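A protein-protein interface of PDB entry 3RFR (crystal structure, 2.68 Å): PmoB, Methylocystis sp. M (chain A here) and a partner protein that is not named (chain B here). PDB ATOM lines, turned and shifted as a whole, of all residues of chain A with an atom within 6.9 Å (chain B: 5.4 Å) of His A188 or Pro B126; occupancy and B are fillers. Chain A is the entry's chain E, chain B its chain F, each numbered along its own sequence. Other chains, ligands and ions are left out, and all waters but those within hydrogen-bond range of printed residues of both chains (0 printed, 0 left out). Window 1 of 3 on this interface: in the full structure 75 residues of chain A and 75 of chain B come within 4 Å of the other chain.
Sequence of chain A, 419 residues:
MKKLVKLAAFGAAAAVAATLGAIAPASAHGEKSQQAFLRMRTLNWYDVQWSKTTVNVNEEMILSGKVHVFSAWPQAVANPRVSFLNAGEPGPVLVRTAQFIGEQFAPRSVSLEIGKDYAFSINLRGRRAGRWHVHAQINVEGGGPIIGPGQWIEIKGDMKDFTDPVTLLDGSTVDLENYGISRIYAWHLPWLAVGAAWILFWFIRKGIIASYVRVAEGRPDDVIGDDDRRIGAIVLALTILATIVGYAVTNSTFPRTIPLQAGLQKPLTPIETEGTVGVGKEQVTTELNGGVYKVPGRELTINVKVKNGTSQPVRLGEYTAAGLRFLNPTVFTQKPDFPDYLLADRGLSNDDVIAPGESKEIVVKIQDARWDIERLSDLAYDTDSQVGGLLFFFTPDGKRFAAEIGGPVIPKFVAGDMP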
ATOM      1  N   ARG A 183     -25.952  33.286   5.984  1.00  0.00           N
ATOM      2  CA  ARG A 183     -27.072  33.390   5.088  1.00  0.00           C
ATOM      3  C   ARG A 183     -27.200  32.068   4.323  1.00  0.00           C
ATOM      4  O   ARG A 183     -28.319  31.625   4.011  1.00  0.00           O
ATOM      5  CB  ARG A 183     -26.846  34.586   4.177  1.00  0.00           C
ATOM      6  CG  ARG A 183     -27.902  34.866   3.178  1.00  0.00           C
ATOM      7  CD  ARG A 183     -27.480  36.026   2.348  1.00  0.00           C
ATOM      8  NE  ARG A 183     -27.792  37.278   3.008  1.00  0.00           N
ATOM      9  CZ  ARG A 183     -28.990  37.843   2.970  1.00  0.00           C
ATOM     10  NH1 ARG A 183     -29.970  37.256   2.306  1.00  0.00           N
ATOM     11  NH2 ARG A 183     -29.211  38.976   3.590  1.00  0.00           N
ATOM     12  N   ILE A 184     -26.058  31.435   4.027  1.00  0.00           N
ATOM     13  CA  ILE A 184     -26.035  30.070   3.491  1.00  0.00           C
ATOM     14  C   ILE A 184     -26.702  29.087   4.461  1.00  0.00           C
ATOM     15  O   ILE A 184     -27.556  28.308   4.051  1.00  0.00           O
ATOM     16  CB  ILE A 184     -24.591  29.640   3.170  1.00  0.00           C
ATOM     17  CG1 ILE A 184     -24.107  30.423   1.980  1.00  0.00           C
ATOM     18  CG2 ILE A 184     -24.438  28.113   2.845  1.00  0.00           C
ATOM     19  CD1 ILE A 184     -22.672  30.785   2.134  1.00  0.00           C
ATOM     20  N   TYR A 185     -26.318  29.127   5.735  1.00  0.00           N
ATOM     21  CA  TYR A 185     -26.925  28.239   6.715  1.00  0.00           C
ATOM     22  C   TYR A 185     -28.414  28.484   6.835  1.00  0.00           C
ATOM     23  O   TYR A 185     -29.191  27.539   6.935  1.00  0.00           O
ATOM     24  CB  TYR A 185     -26.315  28.426   8.101  1.00  0.00           C
ATOM     25  CG  TYR A 185     -24.899  27.947   8.254  1.00  0.00           C
ATOM     26  CD1 TYR A 185     -24.425  26.821   7.565  1.00  0.00           C
ATOM     27  CD2 TYR A 185     -24.039  28.592   9.125  1.00  0.00           C
ATOM     28  CE1 TYR A 185     -23.129  26.376   7.734  1.00  0.00           C
ATOM     29  CE2 TYR A 185     -22.734  28.157   9.285  1.00  0.00           C
ATOM     30  CZ  TYR A 185     -22.286  27.053   8.590  1.00  0.00           C
ATOM     31  OH  TYR A 185     -20.986  26.649   8.782  1.00  0.00           O
ATOM     32  N   ALA A 186     -28.792  29.759   6.843  1.00  0.00           N
ATOM     33  CA  ALA A 186     -30.163  30.186   7.048  1.00  0.00           C
ATOM     34  C   ALA A 186     -31.065  29.673   5.943  1.00  0.00           C
ATOM     35  O   ALA A 186     -32.248  29.467   6.165  1.00  0.00           O
ATOM     36  CB  ALA A 186     -30.240  31.706   7.158  1.00  0.00           C
ATOM     37  N   TRP A 187     -30.503  29.454   4.760  1.00  0.00           N
ATOM     38  CA  TRP A 187     -31.251  28.874   3.649  1.00  0.00           C
ATOM     39  C   TRP A 187     -31.093  27.360   3.554  1.00  0.00           C
ATOM     40  O   TRP A 187     -32.045  26.676   3.261  1.00  0.00           O
ATOM     41  CB  TRP A 187     -30.842  29.534   2.350  1.00  0.00           C
ATOM     42  CG  TRP A 187     -31.590  29.102   1.146  1.00  0.00           C
ATOM     43  CD1 TRP A 187     -31.126  28.326   0.144  1.00  0.00           C
ATOM     44  CD2 TRP A 187     -32.928  29.442   0.804  1.00  0.00           C
ATOM     45  NE1 TRP A 187     -32.089  28.148  -0.813  1.00  0.00           N
ATOM     46  CE2 TRP A 187     -33.210  28.829  -0.436  1.00  0.00           C
ATOM     47  CE3 TRP A 187     -33.927  30.201   1.431  1.00  0.00           C
ATOM     48  CZ2 TRP A 187     -34.449  28.954  -1.077  1.00  0.00           C
ATOM     49  CZ3 TRP A 187     -35.164  30.327   0.795  1.00  0.00           C
ATOM     50  CH2 TRP A 187     -35.412  29.698  -0.449  1.00  0.00           C
ATOM     51  N   HIS A 188     -29.897  26.838   3.809  1.00  0.00           N
ATOM     52  CA  HIS A 188     -29.672  25.395   3.767  1.00  0.00           C
ATOM     53  C   HIS A 188     -30.249  24.633   4.958  1.00  0.00           C
ATOM     54  O   HIS A 188     -30.862  23.589   4.765  1.00  0.00           O
ATOM     55  CB  HIS A 188     -28.198  25.064   3.582  1.00  0.00           C
ATOM     56  CG  HIS A 188     -27.798  24.881   2.150  1.00  0.00           C
ATOM     57  ND1 HIS A 188     -27.633  25.936   1.276  1.00  0.00           N
ATOM     58  CD2 HIS A 188     -27.547  23.763   1.437  1.00  0.00           C
ATOM     59  CE1 HIS A 188     -27.294  25.476   0.091  1.00  0.00           C
ATOM     60  NE2 HIS A 188     -27.232  24.161   0.163  1.00  0.00           N
ATOM     61  N   LEU A 189     -30.089  25.116   6.176  1.00  0.00           N
ATOM     62  CA  LEU A 189     -30.547  24.291   7.277  1.00  0.00           C
ATOM     63  C   LEU A 189     -32.084  24.100   7.338  1.00  0.00           C
ATOM     64  O   LEU A 189     -32.548  22.968   7.492  1.00  0.00           O
ATOM     65  CB  LEU A 189     -29.888  24.679   8.614  1.00  0.00           C
ATOM     66  CG  LEU A 189     -28.332  24.694   8.538  1.00  0.00           C
ATOM     67  CD1 LEU A 189     -27.674  24.811   9.910  1.00  0.00           C
ATOM     68  CD2 LEU A 189     -27.702  23.489   7.783  1.00  0.00           C
ATOM     69  N   PRO A 190     -32.884  25.180   7.179  1.00  0.00           N
ATOM     70  CA  PRO A 190     -34.328  24.907   7.174  1.00  0.00           C
ATOM     71  C   PRO A 190     -34.804  23.923   6.069  1.00  0.00           C
ATOM     72  O   PRO A 190     -35.621  23.044   6.344  1.00  0.00           O
ATOM     73  CB  PRO A 190     -34.945  26.303   7.036  1.00  0.00           C
ATOM     74  CG  PRO A 190     -33.989  27.169   7.751  1.00  0.00           C
ATOM     75  CD  PRO A 190     -32.626  26.626   7.319  1.00  0.00           C
ATOM     76  N   TRP A 191     -34.291  24.039   4.850  1.00  0.00           N
ATOM     77  CA  TRP A 191     -34.664  23.071   3.817  1.00  0.00           C
ATOM     78  C   TRP A 191     -34.262  21.627   4.154  1.00  0.00           C
ATOM     79  O   TRP A 191     -35.084  20.720   3.980  1.00  0.00           O
ATOM     80  CB  TRP A 191     -34.170  23.481   2.437  1.00  0.00           C
ATOM     81  CG  TRP A 191     -34.895  24.615   1.876  1.00  0.00           C
ATOM     82  CD1 TRP A 191     -34.390  25.837   1.637  1.00  0.00           C
ATOM     83  CD2 TRP A 191     -36.283  24.663   1.484  1.00  0.00           C
ATOM     84  NE1 TRP A 191     -35.353  26.662   1.119  1.00  0.00           N
ATOM     85  CE2 TRP A 191     -36.530  25.967   1.008  1.00  0.00           C
ATOM     86  CE3 TRP A 191     -37.340  23.735   1.493  1.00  0.00           C
ATOM     87  CZ2 TRP A 191     -37.807  26.384   0.544  1.00  0.00           C
ATOM     88  CZ3 TRP A 191     -38.623  24.151   1.029  1.00  0.00           C
ATOM     89  CH2 TRP A 191     -38.835  25.469   0.570  1.00  0.00           C
ATOM     90  N   LEU A 192     -33.020  21.430   4.637  1.00  0.00           N
ATOM     91  CA  LEU A 192     -32.593  20.144   5.253  1.00  0.00           C
ATOM     92  C   LEU A 192     -33.613  19.697   6.365  1.00  0.00           C
ATOM     93  O   LEU A 192     -33.957  18.515   6.440  1.00  0.00           O
ATOM     94  CB  LEU A 192     -31.097  20.150   5.738  1.00  0.00           C
ATOM     95  CG  LEU A 192     -29.816  19.730   4.906  1.00  0.00           C
ATOM     96  CD1 LEU A 192     -29.326  20.713   3.868  1.00  0.00           C
ATOM     97  CD2 LEU A 192     -28.621  19.445   5.773  1.00  0.00           C
ATOM     98  N   ALA A 193     -34.136  20.633   7.175  1.00  0.00           N
ATOM     99  CA  ALA A 193     -35.131  20.293   8.215  1.00  0.00           C
ATOM    100  C   ALA A 193     -36.523  19.946   7.645  1.00  0.00           C
ATOM    101  O   ALA A 193     -37.167  18.999   8.101  1.00  0.00           O
ATOM    102  CB  ALA A 193     -35.236  21.403   9.264  1.00  0.00           C
ATOM    103  N   ASP B  54     -20.152  21.079  -7.410  1.00  0.00           N
ATOM    104  CA  ASP B  54     -20.607  21.142  -6.024  1.00  0.00           C
ATOM    105  C   ASP B  54     -19.519  21.602  -5.008  1.00  0.00           C
ATOM    106  O   ASP B  54     -19.786  22.383  -4.090  1.00  0.00           O
ATOM    107  CB  ASP B  54     -21.242  19.824  -5.585  1.00  0.00           C
ATOM    108  CG  ASP B  54     -22.328  20.026  -4.539  1.00  0.00           C
ATOM    109  OD1 ASP B  54     -23.464  20.454  -4.871  1.00  0.00           O
ATOM    110  OD2 ASP B  54     -22.038  19.755  -3.354  1.00  0.00           O
ATOM    111  N   LYS B  60     -19.743  27.519  -9.417  1.00  0.00           N
ATOM    112  CA  LYS B  60     -21.191  27.597  -9.583  1.00  0.00           C
ATOM    113  C   LYS B  60     -21.586  28.753 -10.456  1.00  0.00           C
ATOM    114  O   LYS B  60     -22.034  29.792  -9.921  1.00  0.00           O
ATOM    115  CB  LYS B  60     -21.899  27.757  -8.227  1.00  0.00           C
ATOM    116  CG  LYS B  60     -21.320  26.928  -7.076  1.00  0.00           C
ATOM    117  CD  LYS B  60     -22.387  26.466  -6.180  1.00  0.00           C
ATOM    118  CE  LYS B  60     -21.837  25.706  -4.969  1.00  0.00           C
ATOM    119  NZ  LYS B  60     -20.986  24.611  -5.412  1.00  0.00           N
ATOM    120  N   MET B 102     -27.269  15.767   0.579  1.00  0.00           N
ATOM    121  CA  MET B 102     -27.040  16.952   1.394  1.00  0.00           C
ATOM    122  C   MET B 102     -26.360  16.684   2.719  1.00  0.00           C
ATOM    123  O   MET B 102     -25.411  17.363   3.051  1.00  0.00           O
ATOM    124  CB  MET B 102     -28.349  17.665   1.649  1.00  0.00           C
ATOM    125  CG  MET B 102     -29.021  18.111   0.389  1.00  0.00           C
ATOM    126  SD  MET B 102     -28.063  19.514  -0.082  1.00  0.00           S
ATOM    127  CE  MET B 102     -29.328  20.808   0.166  1.00  0.00           C
ATOM    128  N   GLU B 105     -22.793  15.504   2.225  1.00  0.00           N
ATOM    129  CA  GLU B 105     -21.989  16.637   1.796  1.00  0.00           C
ATOM    130  C   GLU B 105     -21.725  17.561   2.959  1.00  0.00           C
ATOM    131  O   GLU B 105     -20.591  17.744   3.362  1.00  0.00           O
ATOM    132  CB  GLU B 105     -22.643  17.383   0.622  1.00  0.00           C
ATOM    133  CG  GLU B 105     -22.726  16.542  -0.601  1.00  0.00           C
ATOM    134  CD  GLU B 105     -23.394  17.208  -1.758  1.00  0.00           C
ATOM    135  OE1 GLU B 105     -24.303  18.031  -1.517  1.00  0.00           O
ATOM    136  OE2 GLU B 105     -23.021  16.885  -2.931  1.00  0.00           O
ATOM    137  N   TRP B 106     -22.781  18.111   3.530  1.00  0.00           N
ATOM    138  CA  TRP B 106     -22.636  19.087   4.602  1.00  0.00           C
ATOM    139  C   TRP B 106     -21.750  18.631   5.748  1.00  0.00           C
ATOM    140  O   TRP B 106     -20.890  19.407   6.206  1.00  0.00           O
ATOM    141  CB  TRP B 106     -23.991  19.573   5.111  1.00  0.00           C
ATOM    142  CG  TRP B 106     -24.440  20.873   4.489  1.00  0.00           C
ATOM    143  CD1 TRP B 106     -25.528  21.059   3.714  1.00  0.00           C
ATOM    144  CD2 TRP B 106     -23.798  22.158   4.590  1.00  0.00           C
ATOM    145  NE1 TRP B 106     -25.630  22.369   3.331  1.00  0.00           N
ATOM    146  CE2 TRP B 106     -24.588  23.071   3.862  1.00  0.00           C
ATOM    147  CE3 TRP B 106     -22.654  22.634   5.266  1.00  0.00           C
ATOM    148  CZ2 TRP B 106     -24.267  24.440   3.761  1.00  0.00           C
ATOM    149  CZ3 TRP B 106     -22.336  24.000   5.184  1.00  0.00           C
ATOM    150  CH2 TRP B 106     -23.138  24.884   4.427  1.00  0.00           C
ATOM    151  N   ARG B 109     -18.224  19.088   4.404  1.00  0.00           N
ATOM    152  CA  ARG B 109     -17.728  20.447   4.191  1.00  0.00           C
ATOM    153  C   ARG B 109     -17.367  21.058   5.544  1.00  0.00           C
ATOM    154  O   ARG B 109     -16.331  21.701   5.713  1.00  0.00           O
ATOM    155  CB  ARG B 109     -18.739  21.322   3.423  1.00  0.00           C
ATOM    156  CG  ARG B 109     -19.392  20.685   2.184  1.00  0.00           C
ATOM    157  CD  ARG B 109     -18.371  20.234   1.224  1.00  0.00           C
ATOM    158  NE  ARG B 109     -18.861  19.315   0.210  1.00  0.00           N
ATOM    159  CZ  ARG B 109     -19.407  19.691  -0.951  1.00  0.00           C
ATOM    160  NH1 ARG B 109     -19.603  20.974  -1.226  1.00  0.00           N
ATOM    161  NH2 ARG B 109     -19.764  18.778  -1.849  1.00  0.00           N
ATOM    162  N   VAL B 124     -16.963  26.274   0.095  1.00  0.00           N
ATOM    163  CA  VAL B 124     -17.094  24.841  -0.117  1.00  0.00           C
ATOM    164  C   VAL B 124     -18.480  24.315   0.092  1.00  0.00           C
ATOM    165  O   VAL B 124     -18.646  23.103   0.090  1.00  0.00           O
ATOM    166  CB  VAL B 124     -16.129  24.043   0.771  1.00  0.00           C
ATOM    167  CG1 VAL B 124     -14.677  24.333   0.386  1.00  0.00           C
ATOM    168  CG2 VAL B 124     -16.395  24.332   2.317  1.00  0.00           C
ATOM    169  N   PHE B 125     -19.473  25.196   0.246  1.00  0.00           N
ATOM    170  CA  PHE B 125     -20.840  24.759   0.543  1.00  0.00           C
ATOM    171  C   PHE B 125     -21.524  24.129  -0.662  1.00  0.00           C
ATOM    172  O   PHE B 125     -21.247  24.532  -1.779  1.00  0.00           O
ATOM    173  CB  PHE B 125     -21.669  25.908   1.074  1.00  0.00           C
ATOM    174  CG  PHE B 125     -21.955  27.015   0.052  1.00  0.00           C
ATOM    175  CD1 PHE B 125     -23.080  26.952  -0.797  1.00  0.00           C
ATOM    176  CD2 PHE B 125     -21.143  28.162   0.009  1.00  0.00           C
ATOM    177  CE1 PHE B 125     -23.361  27.978  -1.676  1.00  0.00           C
ATOM    178  CE2 PHE B 125     -21.423  29.203  -0.893  1.00  0.00           C
ATOM    179  CZ  PHE B 125     -22.519  29.112  -1.725  1.00  0.00           C
ATOM    180  N   PRO B 126     -22.452  23.165  -0.428  1.00  0.00           N
ATOM    181  CA  PRO B 126     -23.017  22.332  -1.487  1.00  0.00           C
ATOM    182  C   PRO B 126     -24.193  22.990  -2.217  1.00  0.00           C
ATOM    183  O   PRO B 126     -24.749  23.974  -1.713  1.00  0.00           O
ATOM    184  CB  PRO B 126     -23.505  21.108  -0.716  1.00  0.00           C
ATOM    185  CG  PRO B 126     -23.856  21.602   0.598  1.00  0.00           C
ATOM    186  CD  PRO B 126     -23.014  22.795   0.890  1.00  0.00           C
ATOM    187  N   SER B 127     -24.560  22.445  -3.384  1.00  0.00           N
ATOM    188  CA  SER B 127     -25.733  22.918  -4.120  1.00  0.00           C
ATOM    189  C   SER B 127     -27.053  22.532  -3.442  1.00  0.00           C
ATOM    190  O   SER B 127     -27.234  21.416  -2.952  1.00  0.00           O
ATOM    191  CB  SER B 127     -25.751  22.412  -5.547  1.00  0.00           C
ATOM    192  OG  SER B 127     -24.455  22.379  -6.089  1.00  0.00           O
ATOM    193  N   ALA B 128     -27.969  23.495  -3.448  1.00  0.00           N
ATOM    194  CA  ALA B 128     -29.288  23.365  -2.873  1.00  0.00           C
ATOM    195  C   ALA B 128     -30.151  22.417  -3.705  1.00  0.00           C
ATOM    196  O   ALA B 128     -30.322  22.607  -4.919  1.00  0.00           O
ATOM    197  CB  ALA B 128     -29.899  24.747  -2.809  1.00  0.00           C
ATOM    198  N   ASN B 165     -31.275  27.896  -5.552  1.00  0.00           N
ATOM    199  CA  ASN B 165     -29.877  28.129  -5.192  1.00  0.00           C
ATOM    200  C   ASN B 165     -29.506  29.582  -4.986  1.00  0.00           C
ATOM    201  O   ASN B 165     -28.650  29.908  -4.151  1.00  0.00           O
ATOM    202  CB  ASN B 165     -28.957  27.501  -6.225  1.00  0.00           C
ATOM    203  CG  ASN B 165     -28.647  26.081  -5.889  1.00  0.00           C
ATOM    204  OD1 ASN B 165     -27.956  25.812  -4.889  1.00  0.00           O
ATOM    205  ND2 ASN B 165     -29.222  25.146  -6.655  1.00  0.00           N
ATOM    206  N   ALA B 168     -28.611  31.386  -1.570  1.00  0.00           N
ATOM    207  CA  ALA B 168     -27.359  30.961  -0.937  1.00  0.00           C
ATOM    208  C   ALA B 168     -26.142  31.503  -1.663  1.00  0.00           C
ATOM    209  O   ALA B 168     -25.058  31.580  -1.099  1.00  0.00           O
ATOM    210  CB  ALA B 168     -27.294  29.451  -0.946  1.00  0.00           C
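OD1 of Asp B54 is in hydrogen-bond range of OG of Ser B127 (2.5 Å). The backbone NH (N) of Ala B128 sits at hydrogen-bond distance from the side-chain amide oxygen (OD1) of Asn B165 (2.7 Å).
Of chain B, only Met B102, Trp B106, Pro B126, Ser B127 and Ala B128 come within 4 Å of His A188. Of the printed residues of chain A, Pro B126 touches His A188. Printed residues of chain A within 4 Å of Ser B127: His A188. Printed residues of chain A within 4 Å of Phe B125: Ile A184. Ala A186 touches none of the printed residues of chain B. Arg B109 touches none of the printed residues of chain A. The nearest residue of chain B that does not touch His A188 is Ala B168 (4.1 Å).
A ring nitrogen (NE2) of His A188 lies within hydrogen-bond range of the backbone carbonyl oxygen (O) of Pro B126, at 3.1 Å.
Among the printed residues, pairs that only touch across the chains: His A188 with Trp B106, Ile A184 with Ala B168, Tyr A185 with Trp B106, Ile A184 with Phe B125, His A188 with Met B102, Leu A192 with Met B102, His A188 with Ala B128, Ile A184 with Trp B106, Leu A192 with Trp B106 and His A188 with Ser B127.
Of the 13 printed residues of chain B, 7 touch a printed residue of chain A. Hydrophobic or aromatic side chains of chain B within 4 Å of the printed part of chain A: Met B102, Trp B106, Phe B125 and Ala B128. Of the 11 printed residues of chain A, 4 touch a printed residue of chain B. Printed residues of chain A that touch a printed residue of chain B: Ile A184, Tyr A185, His A188 and Leu A192. Hydrophobic or aromatic side chains of chain A within 4 Å of the printed part of chain B: Ile A184, Tyr A185, His A188 and Leu A192. Along chain A the printed residues that touch a printed residue of chain B span positions 184 to 192.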
